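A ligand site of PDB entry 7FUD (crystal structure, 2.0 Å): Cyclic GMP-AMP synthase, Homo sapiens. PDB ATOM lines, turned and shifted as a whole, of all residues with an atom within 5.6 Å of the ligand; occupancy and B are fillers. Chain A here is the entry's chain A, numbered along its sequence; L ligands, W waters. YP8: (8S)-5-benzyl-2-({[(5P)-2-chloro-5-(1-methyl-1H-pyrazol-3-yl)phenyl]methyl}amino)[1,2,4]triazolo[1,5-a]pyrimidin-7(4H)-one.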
ATOM      1  N   ARG A  86      12.207  -1.890 -22.957  1.00  0.00           N
ATOM      2  CA  ARG A  86      11.341  -0.735 -22.728  1.00  0.00           C
ATOM      3  C   ARG A  86      10.504  -0.868 -21.452  1.00  0.00           C
ATOM      4  O   ARG A  86       9.940   0.131 -20.987  1.00  0.00           O
ATOM      5  CB  ARG A  86      10.440  -0.483 -23.948  1.00  0.00           C
ATOM      6  CG  ARG A  86      11.186  -0.250 -25.278  1.00  0.00           C
ATOM      7  CD  ARG A  86      11.356   1.238 -25.619  1.00  0.00           C
ATOM      8  NE  ARG A  86      12.192   1.962 -24.661  1.00  0.00           N
ATOM      9  CZ  ARG A  86      12.282   3.298 -24.582  1.00  0.00           C
ATOM     10  NH1 ARG A  86      11.589   4.066 -25.420  1.00  0.00           N
ATOM     11  NH2 ARG A  86      13.064   3.867 -23.665  1.00  0.00           N
ATOM     12  N   ALA A  87      10.442  -2.065 -20.859  1.00  0.00           N
ATOM     13  CA  ALA A  87       9.601  -2.297 -19.686  1.00  0.00           C
ATOM     14  C   ALA A  87      10.324  -2.932 -18.497  1.00  0.00           C
ATOM     15  O   ALA A  87       9.886  -2.774 -17.353  1.00  0.00           O
ATOM     16  CB  ALA A  87       8.433  -3.189 -20.074  1.00  0.00           C
ATOM     17  N   TYR A  88      11.409  -3.651 -18.736  1.00  0.00           N
ATOM     18  CA  TYR A  88      12.117  -4.333 -17.674  1.00  0.00           C
ATOM     19  C   TYR A  88      13.390  -3.561 -17.326  1.00  0.00           C
ATOM     20  O   TYR A  88      14.087  -3.071 -18.220  1.00  0.00           O
ATOM     21  CB  TYR A  88      12.431  -5.788 -18.105  1.00  0.00           C
ATOM     22  CG  TYR A  88      11.168  -6.622 -18.337  1.00  0.00           C
ATOM     23  CD1 TYR A  88      10.514  -6.590 -19.561  1.00  0.00           C
ATOM     24  CD2 TYR A  88      10.618  -7.394 -17.304  1.00  0.00           C
ATOM     25  CE1 TYR A  88       9.346  -7.330 -19.769  1.00  0.00           C
ATOM     26  CE2 TYR A  88       9.451  -8.134 -17.512  1.00  0.00           C
ATOM     27  CZ  TYR A  88       8.826  -8.092 -18.747  1.00  0.00           C
ATOM     28  OH  TYR A  88       7.667  -8.819 -18.975  1.00  0.00           O
ATOM     29  N   LYS A 202       9.888  -9.514 -12.087  1.00  0.00           N
ATOM     30  CA  LYS A 202       9.483 -10.378 -13.198  1.00  0.00           C
ATOM     31  C   LYS A 202      10.624 -10.579 -14.185  1.00  0.00           C
ATOM     32  O   LYS A 202      11.273  -9.614 -14.600  1.00  0.00           O
ATOM     33  CB  LYS A 202       8.255  -9.814 -13.920  1.00  0.00           C
ATOM     34  CG  LYS A 202       7.583 -10.808 -14.857  1.00  0.00           C
ATOM     35  CD  LYS A 202       6.527 -10.114 -15.723  1.00  0.00           C
ATOM     36  CE  LYS A 202       6.079 -11.025 -16.856  1.00  0.00           C
ATOM     37  NZ  LYS A 202       4.942 -10.427 -17.639  1.00  0.00           N
ATOM     38  N   ARG A 216       9.687  -5.053 -13.587  1.00  0.00           N
ATOM     39  CA  ARG A 216       8.797  -4.607 -14.644  1.00  0.00           C
ATOM     40  C   ARG A 216       8.020  -3.403 -14.139  1.00  0.00           C
ATOM     41  O   ARG A 216       7.561  -3.395 -12.998  1.00  0.00           O
ATOM     42  CB  ARG A 216       7.838  -5.738 -15.033  1.00  0.00           C
ATOM     43  CG  ARG A 216       6.678  -5.340 -15.916  1.00  0.00           C
ATOM     44  CD  ARG A 216       5.722  -6.514 -16.181  1.00  0.00           C
ATOM     45  NE  ARG A 216       4.889  -6.945 -15.042  1.00  0.00           N
ATOM     46  CZ  ARG A 216       3.981  -6.194 -14.394  1.00  0.00           C
ATOM     47  NH1 ARG A 216       3.770  -4.916 -14.701  1.00  0.00           N
ATOM     48  NH2 ARG A 216       3.289  -6.735 -13.405  1.00  0.00           N
ATOM     49  N   LEU A 217       7.914  -2.367 -14.968  1.00  0.00           N
ATOM     50  CA  LEU A 217       7.133  -1.214 -14.548  1.00  0.00           C
ATOM     51  C   LEU A 217       5.682  -1.632 -14.268  1.00  0.00           C
ATOM     52  O   LEU A 217       5.130  -2.508 -14.934  1.00  0.00           O
ATOM     53  CB  LEU A 217       7.168  -0.127 -15.625  1.00  0.00           C
ATOM     54  CG  LEU A 217       8.536   0.523 -15.880  1.00  0.00           C
ATOM     55  CD1 LEU A 217       8.515   1.359 -17.130  1.00  0.00           C
ATOM     56  CD2 LEU A 217       8.915   1.382 -14.708  1.00  0.00           C
ATOM     57  N   SER A 218       5.071  -0.979 -13.279  1.00  0.00           N
ATOM     58  CA  SER A 218       3.709  -1.291 -12.889  1.00  0.00           C
ATOM     59  C   SER A 218       2.938   0.007 -12.709  1.00  0.00           C
ATOM     60  O   SER A 218       3.442   0.953 -12.124  1.00  0.00           O
ATOM     61  CB  SER A 218       3.649  -2.099 -11.593  1.00  0.00           C
ATOM     62  OG  SER A 218       2.305  -2.377 -11.240  1.00  0.00           O
ATOM     63  N   PHE A 219       1.715   0.038 -13.242  1.00  0.00           N
ATOM     64  CA  PHE A 219       0.798   1.156 -13.121  1.00  0.00           C
ATOM     65  C   PHE A 219      -0.556   0.647 -12.672  1.00  0.00           C
ATOM     66  O   PHE A 219      -1.585   0.911 -13.287  1.00  0.00           O
ATOM     67  CB  PHE A 219       0.672   1.913 -14.436  1.00  0.00           C
ATOM     68  CG  PHE A 219       1.961   2.480 -14.927  1.00  0.00           C
ATOM     69  CD1 PHE A 219       2.366   3.741 -14.532  1.00  0.00           C
ATOM     70  CD2 PHE A 219       2.792   1.752 -15.771  1.00  0.00           C
ATOM     71  CE1 PHE A 219       3.564   4.267 -14.978  1.00  0.00           C
ATOM     72  CE2 PHE A 219       3.984   2.269 -16.225  1.00  0.00           C
ATOM     73  CZ  PHE A 219       4.373   3.539 -15.816  1.00  0.00           C
ATOM     74  N   SER A 220      -0.543  -0.095 -11.549  1.00  0.00           N
ATOM     75  CA  SER A 220      -1.733  -0.732 -11.007  1.00  0.00           C
ATOM     76  C   SER A 220      -2.767   0.262 -10.522  1.00  0.00           C
ATOM     77  O   SER A 220      -3.942  -0.100 -10.393  1.00  0.00           O
ATOM     78  CB  SER A 220      -1.370  -1.634  -9.823  1.00  0.00           C
ATOM     79  OG  SER A 220      -0.866  -2.871 -10.295  1.00  0.00           O
ATOM     80  N   ILE A 222      -3.627   3.253 -11.866  1.00  0.00           N
ATOM     81  CA  ILE A 222      -4.153   4.246 -12.804  1.00  0.00           C
ATOM     82  C   ILE A 222      -5.604   3.952 -13.131  1.00  0.00           C
ATOM     83  O   ILE A 222      -6.466   4.840 -13.036  1.00  0.00           O
ATOM     84  CB  ILE A 222      -3.285   4.315 -14.062  1.00  0.00           C
ATOM     85  CG1 ILE A 222      -1.908   4.815 -13.656  1.00  0.00           C
ATOM     86  CG2 ILE A 222      -3.907   5.298 -15.051  1.00  0.00           C
ATOM     87  CD1 ILE A 222      -1.950   6.141 -12.946  1.00  0.00           C
ATOM     88  N   GLU A 223      -5.893   2.689 -13.453  1.00  0.00           N
ATOM     89  CA  GLU A 223      -7.206   2.272 -13.904  1.00  0.00           C
ATOM     90  C   GLU A 223      -8.315   2.780 -12.983  1.00  0.00           C
ATOM     91  O   GLU A 223      -9.307   3.338 -13.445  1.00  0.00           O
ATOM     92  CB  GLU A 223      -7.260   0.736 -14.015  1.00  0.00           C
ATOM     93  CG  GLU A 223      -8.671   0.153 -14.098  1.00  0.00           C
ATOM     94  CD  GLU A 223      -8.675  -1.374 -14.119  1.00  0.00           C
ATOM     95  OE1 GLU A 223      -9.745  -1.968 -14.405  1.00  0.00           O
ATOM     96  OE2 GLU A 223      -7.622  -1.994 -13.851  1.00  0.00           O
ATOM     97  N   ILE A 226      -9.090   6.391 -13.558  1.00  0.00           N
ATOM     98  CA  ILE A 226      -9.796   6.688 -14.795  1.00  0.00           C
ATOM     99  C   ILE A 226     -11.215   6.132 -14.747  1.00  0.00           C
ATOM    100  O   ILE A 226     -12.146   6.779 -15.210  1.00  0.00           O
ATOM    101  CB  ILE A 226      -8.999   6.116 -15.960  1.00  0.00           C
ATOM    102  CG1 ILE A 226      -7.743   6.943 -16.228  1.00  0.00           C
ATOM    103  CG2 ILE A 226      -9.879   6.017 -17.193  1.00  0.00           C
ATOM    104  CD1 ILE A 226      -6.847   6.177 -17.213  1.00  0.00           C
ATOM    105  N   TYR A 276      -5.580  -7.813 -18.100  1.00  0.00           N
ATOM    106  CA  TYR A 276      -4.947  -6.565 -18.516  1.00  0.00           C
ATOM    107  C   TYR A 276      -4.826  -6.462 -20.029  1.00  0.00           C
ATOM    108  O   TYR A 276      -4.676  -5.349 -20.524  1.00  0.00           O
ATOM    109  CB  TYR A 276      -3.596  -6.364 -17.849  1.00  0.00           C
ATOM    110  CG  TYR A 276      -2.454  -7.095 -18.484  1.00  0.00           C
ATOM    111  CD1 TYR A 276      -2.268  -8.452 -18.273  1.00  0.00           C
ATOM    112  CD2 TYR A 276      -1.508  -6.414 -19.261  1.00  0.00           C
ATOM    113  CE1 TYR A 276      -1.200  -9.137 -18.838  1.00  0.00           C
ATOM    114  CE2 TYR A 276      -0.426  -7.090 -19.824  1.00  0.00           C
ATOM    115  CZ  TYR A 276      -0.283  -8.455 -19.617  1.00  0.00           C
ATOM    116  OH  TYR A 276       0.776  -9.162 -20.163  1.00  0.00           O
ATOM    117  N   LYS A 279      -8.195  -4.799 -20.583  1.00  0.00           N
ATOM    118  CA  LYS A 279      -8.154  -3.393 -20.187  1.00  0.00           C
ATOM    119  C   LYS A 279      -7.363  -2.555 -21.167  1.00  0.00           C
ATOM    120  O   LYS A 279      -7.810  -1.488 -21.591  1.00  0.00           O
ATOM    121  CB  LYS A 279      -7.554  -3.270 -18.788  1.00  0.00           C
ATOM    122  CG  LYS A 279      -8.350  -3.917 -17.711  1.00  0.00           C
ATOM    123  CD  LYS A 279      -7.574  -3.972 -16.409  1.00  0.00           C
ATOM    124  CE  LYS A 279      -8.283  -4.865 -15.414  1.00  0.00           C
ATOM    125  NZ  LYS A 279      -7.912  -4.470 -14.033  1.00  0.00           N
ATOM    126  N   THR A 280      -6.171  -3.031 -21.558  1.00  0.00           N
ATOM    127  CA  THR A 280      -5.391  -2.302 -22.557  1.00  0.00           C
ATOM    128  C   THR A 280      -6.247  -2.010 -23.784  1.00  0.00           C
ATOM    129  O   THR A 280      -6.385  -0.855 -24.197  1.00  0.00           O
ATOM    130  CB  THR A 280      -4.143  -3.094 -22.933  1.00  0.00           C
ATOM    131  OG1 THR A 280      -3.346  -3.327 -21.754  1.00  0.00           O
ATOM    132  CG2 THR A 280      -3.340  -2.333 -23.948  1.00  0.00           C
ATOM    133  N   PHE A 283      -9.203   0.518 -23.141  1.00  0.00           N
ATOM    134  CA  PHE A 283      -8.816   1.919 -23.018  1.00  0.00           C
ATOM    135  C   PHE A 283      -8.291   2.490 -24.324  1.00  0.00           C
ATOM    136  O   PHE A 283      -8.411   3.696 -24.559  1.00  0.00           O
ATOM    137  CB  PHE A 283      -7.826   2.086 -21.884  1.00  0.00           C
ATOM    138  CG  PHE A 283      -8.474   2.009 -20.538  1.00  0.00           C
ATOM    139  CD1 PHE A 283      -9.361   2.985 -20.129  1.00  0.00           C
ATOM    140  CD2 PHE A 283      -8.243   0.937 -19.702  1.00  0.00           C
ATOM    141  CE1 PHE A 283      -9.980   2.918 -18.886  1.00  0.00           C
ATOM    142  CE2 PHE A 283      -8.869   0.869 -18.453  1.00  0.00           C
ATOM    143  CZ  PHE A 283      -9.732   1.866 -18.062  1.00  0.00           C
ATOM    144  N   ASN A 322       1.057  -1.543 -25.367  1.00  0.00           N
ATOM    145  CA  ASN A 322       0.845  -1.281 -23.952  1.00  0.00           C
ATOM    146  C   ASN A 322       0.372   0.176 -23.769  1.00  0.00           C
ATOM    147  O   ASN A 322       0.813   1.071 -24.492  1.00  0.00           O
ATOM    148  CB  ASN A 322       2.132  -1.562 -23.175  1.00  0.00           C
ATOM    149  CG  ASN A 322       1.973  -1.297 -21.713  1.00  0.00           C
ATOM    150  OD1 ASN A 322       2.134  -0.162 -21.271  1.00  0.00           O
ATOM    151  ND2 ASN A 322       1.643  -2.341 -20.947  1.00  0.00           N
ATOM    152  N   TYR A 323      -0.566   0.395 -22.835  1.00  0.00           N
ATOM    153  CA  TYR A 323      -1.194   1.707 -22.750  1.00  0.00           C
ATOM    154  C   TYR A 323      -0.221   2.771 -22.302  1.00  0.00           C
ATOM    155  O   TYR A 323      -0.399   3.950 -22.638  1.00  0.00           O
ATOM    156  CB  TYR A 323      -2.367   1.688 -21.766  1.00  0.00           C
ATOM    157  CG  TYR A 323      -3.382   2.746 -22.086  1.00  0.00           C
ATOM    158  CD1 TYR A 323      -4.084   2.697 -23.293  1.00  0.00           C
ATOM    159  CD2 TYR A 323      -3.685   3.770 -21.192  1.00  0.00           C
ATOM    160  CE1 TYR A 323      -5.040   3.652 -23.612  1.00  0.00           C
ATOM    161  CE2 TYR A 323      -4.655   4.734 -21.497  1.00  0.00           C
ATOM    162  CZ  TYR A 323      -5.315   4.675 -22.716  1.00  0.00           C
ATOM    163  OH  TYR A 323      -6.256   5.610 -23.050  1.00  0.00           O
ATOM    164  N   PHE A 324       0.792   2.392 -21.543  1.00  0.00           N
ATOM    165  CA  PHE A 324       1.732   3.307 -20.913  1.00  0.00           C
ATOM    166  C   PHE A 324       3.039   3.379 -21.674  1.00  0.00           C
ATOM    167  O   PHE A 324       3.571   4.467 -21.879  1.00  0.00           O
ATOM    168  CB  PHE A 324       1.961   2.864 -19.458  1.00  0.00           C
ATOM    169  CG  PHE A 324       0.702   2.914 -18.616  1.00  0.00           C
ATOM    170  CD1 PHE A 324       0.313   4.091 -17.999  1.00  0.00           C
ATOM    171  CD2 PHE A 324      -0.123   1.805 -18.494  1.00  0.00           C
ATOM    172  CE1 PHE A 324      -0.853   4.146 -17.249  1.00  0.00           C
ATOM    173  CE2 PHE A 324      -1.295   1.871 -17.751  1.00  0.00           C
ATOM    174  CZ  PHE A 324      -1.651   3.045 -17.110  1.00  0.00           C
ATOM    175  N   ILE A 325       3.513   2.245 -22.160  1.00  0.00           N
ATOM    176  CA  ILE A 325       4.744   2.140 -22.945  1.00  0.00           C
ATOM    177  C   ILE A 325       4.346   1.730 -24.358  1.00  0.00           C
ATOM    178  O   ILE A 325       4.228   0.528 -24.661  1.00  0.00           O
ATOM    179  CB  ILE A 325       5.701   1.130 -22.290  1.00  0.00           C
ATOM    180  CG1 ILE A 325       5.858   1.502 -20.807  1.00  0.00           C
ATOM    181  CG2 ILE A 325       7.030   1.058 -23.035  1.00  0.00           C
ATOM    182  CD1 ILE A 325       6.671   0.521 -19.995  1.00  0.00           C
ATOM    183  N   PHE A 328       5.870  -1.160 -26.509  1.00  0.00           N
ATOM    184  CA  PHE A 328       5.816  -2.536 -26.041  1.00  0.00           C
ATOM    185  C   PHE A 328       4.579  -3.204 -26.618  1.00  0.00           C
ATOM    186  O   PHE A 328       3.452  -2.813 -26.295  1.00  0.00           O
ATOM    187  CB  PHE A 328       5.808  -2.625 -24.518  1.00  0.00           C
ATOM    188  CG  PHE A 328       6.112  -4.028 -24.003  1.00  0.00           C
ATOM    189  CD1 PHE A 328       5.123  -4.999 -23.986  1.00  0.00           C
ATOM    190  CD2 PHE A 328       7.371  -4.362 -23.569  1.00  0.00           C
ATOM    191  CE1 PHE A 328       5.402  -6.294 -23.540  1.00  0.00           C
ATOM    192  CE2 PHE A 328       7.656  -5.658 -23.116  1.00  0.00           C
ATOM    193  CZ  PHE A 328       6.668  -6.628 -23.113  1.00  0.00           C
ATOM    194  N   LEU A 330       2.083  -6.056 -26.646  1.00  0.00           N
ATOM    195  CA  LEU A 330       1.672  -7.158 -25.778  1.00  0.00           C
ATOM    196  C   LEU A 330       1.320  -8.408 -26.588  1.00  0.00           C
ATOM    197  O   LEU A 330       1.314  -9.494 -26.015  1.00  0.00           O
ATOM    198  CB  LEU A 330       0.492  -6.733 -24.899  1.00  0.00           C
ATOM    199  CG  LEU A 330       0.552  -5.539 -23.924  1.00  0.00           C
ATOM    200  CD1 LEU A 330      -0.863  -5.296 -23.346  1.00  0.00           C
ATOM    201  CD2 LEU A 330       1.586  -5.732 -22.745  1.00  0.00           C
HETATM  202  C10 YP8 L   1      -2.382  -2.104 -17.264  1.00  0.00           C
HETATM  203  C15 YP8 L   1       3.273  -4.288 -18.118  1.00  0.00           C
HETATM  204  C16 YP8 L   1       3.365  -5.616 -18.539  1.00  0.00           C
HETATM  205  C17 YP8 L   1       4.135  -5.919 -19.658  1.00  0.00           C
HETATM  206  C18 YP8 L   1       4.784  -4.925 -20.348  1.00  0.00           C
HETATM  207  C19 YP8 L   1       4.676  -3.618 -19.916  1.00  0.00           C
HETATM  208  C21 YP8 L   1       2.660  -6.692 -17.812  1.00  0.00           C
HETATM  209  C22 YP8 L   1       2.653  -8.073 -18.075  1.00  0.00           C
HETATM  210  C23 YP8 L   1       1.855  -8.618 -17.101  1.00  0.00           C
HETATM  211  C26 YP8 L   1       0.571  -7.657 -15.156  1.00  0.00           C
HETATM  212  C27 YP8 L   1      -4.264  -0.752 -18.070  1.00  0.00           C
HETATM  213  C28 YP8 L   1      -4.374  -0.116 -19.296  1.00  0.00           C
HETATM  214  C1  YP8 L   1       3.929  -3.265 -18.797  1.00  0.00           C
HETATM  215  C12 YP8 L   1      -0.036  -1.802 -17.429  1.00  0.00           C
HETATM  216  C14 YP8 L   1      -3.710  -2.151 -17.970  1.00  0.00           C
HETATM  217  C2  YP8 L   1       3.852  -1.796 -18.383  1.00  0.00           C
HETATM  218  C29 YP8 L   1      -4.891   1.171 -19.391  1.00  0.00           C
HETATM  219  C30 YP8 L   1      -5.298   1.832 -18.257  1.00  0.00           C
HETATM  220  C31 YP8 L   1      -5.210   1.206 -17.024  1.00  0.00           C
HETATM  221  C32 YP8 L   1      -4.700  -0.079 -16.937  1.00  0.00           C
HETATM  222  C4  YP8 L   1       1.946  -1.652 -16.876  1.00  0.00           C
HETATM  223  C7  YP8 L   1      -1.012  -2.286 -15.244  1.00  0.00           C
HETATM  224  C9  YP8 L   1      -2.263  -2.319 -15.922  1.00  0.00           C
HETATM  225  N11 YP8 L   1      -1.265  -1.825 -18.018  1.00  0.00           N
HETATM  226  N13 YP8 L   1       1.135  -1.577 -17.972  1.00  0.00           N
HETATM  227  N24 YP8 L   1       1.433  -7.596 -16.331  1.00  0.00           N
HETATM  228  N25 YP8 L   1       1.915  -6.394 -16.741  1.00  0.00           N
HETATM  229  N3  YP8 L   1       3.266  -1.509 -17.080  1.00  0.00           N
HETATM  230  N5  YP8 L   1       1.374  -1.923 -15.714  1.00  0.00           N
HETATM  231  N6  YP8 L   1       0.064  -2.014 -16.110  1.00  0.00           N
HETATM  232  O8  YP8 L   1      -0.809  -2.469 -14.050  1.00  0.00           O
HETATM  233 CL20 YP8 L   1       5.486  -2.387 -20.819  1.00  0.00          CL
HETATM  234  O   HOH W   1      -1.458  -1.655 -20.910  1.00  0.00           O
HETATM  235  O   HOH W   2      -2.434  -4.002 -13.148  1.00  0.00           O
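N13 of the ligand lies within hydrogen-bond range of ND2 of Asn 322 (3.1 Å). A nitrogen (N5) of the ligand sits at hydrogen-bond distance from the backbone NH of Phe 219, at 3.2 Å. An oxygen (O8) of the ligand sits at hydrogen-bond distance from the backbone NH (N) of Ser 220 (3.5 Å). A nitrogen (N25) of the ligand lies within hydrogen-bond range of the guanidinium group (NH1) of Arg 216, 3.1 Å away. N3 of the ligand lies within hydrogen-bond range of O of Leu 217 (3.0 Å).
OD1 of Asn 322 lies within hydrogen-bond range of N of Phe 324 (2.9 Å). The side-chain amino group of Lys 279 lies within salt-bridge range of the side-chain carboxylate of Glu 223 (2.5 Å). OD1 of Asn 322 lies within hydrogen-bond range of N of Ile 325 (2.9 Å). The backbone carbonyl oxygen of Phe 283 sits at hydrogen-bond distance from the side-chain hydroxyl of Tyr 323, 3.3 Å away. The backbone NH of Asn 322 is in hydrogen-bond range of the backbone carbonyl oxygen of Phe 328 (2.9 Å). NZ of Lys 202 sits at hydrogen-bond distance from OH of Tyr 88, 3.4 Å away. N of Leu 217 is in hydrogen-bond range of O of Ala 87 (3.1 Å). The backbone carbonyl oxygen of Tyr 276 lies within hydrogen-bond range of the side-chain hydroxyl of Thr 280 (2.7 Å).
Residues that only touch the ligand: Ala 87, Lys 202, Ser 218, Glu 223, Tyr 276, Thr 280, Phe 283, Tyr 323, Phe 324, Ile 325 and Phe 328. Hydrophobic or aromatic side chains within 4 Å of the ligand: Ala 87, Phe 219, Tyr 276, Phe 283, Tyr 323, Phe 324, Ile 325 and Phe 328. Of the 22 residues printed, 16 come within 4 Å of the ligand.
Water W2 lies within hydrogen-bond range of an oxygen (O8) of the ligand and the side-chain hydroxyl (OG) of Ser 220.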
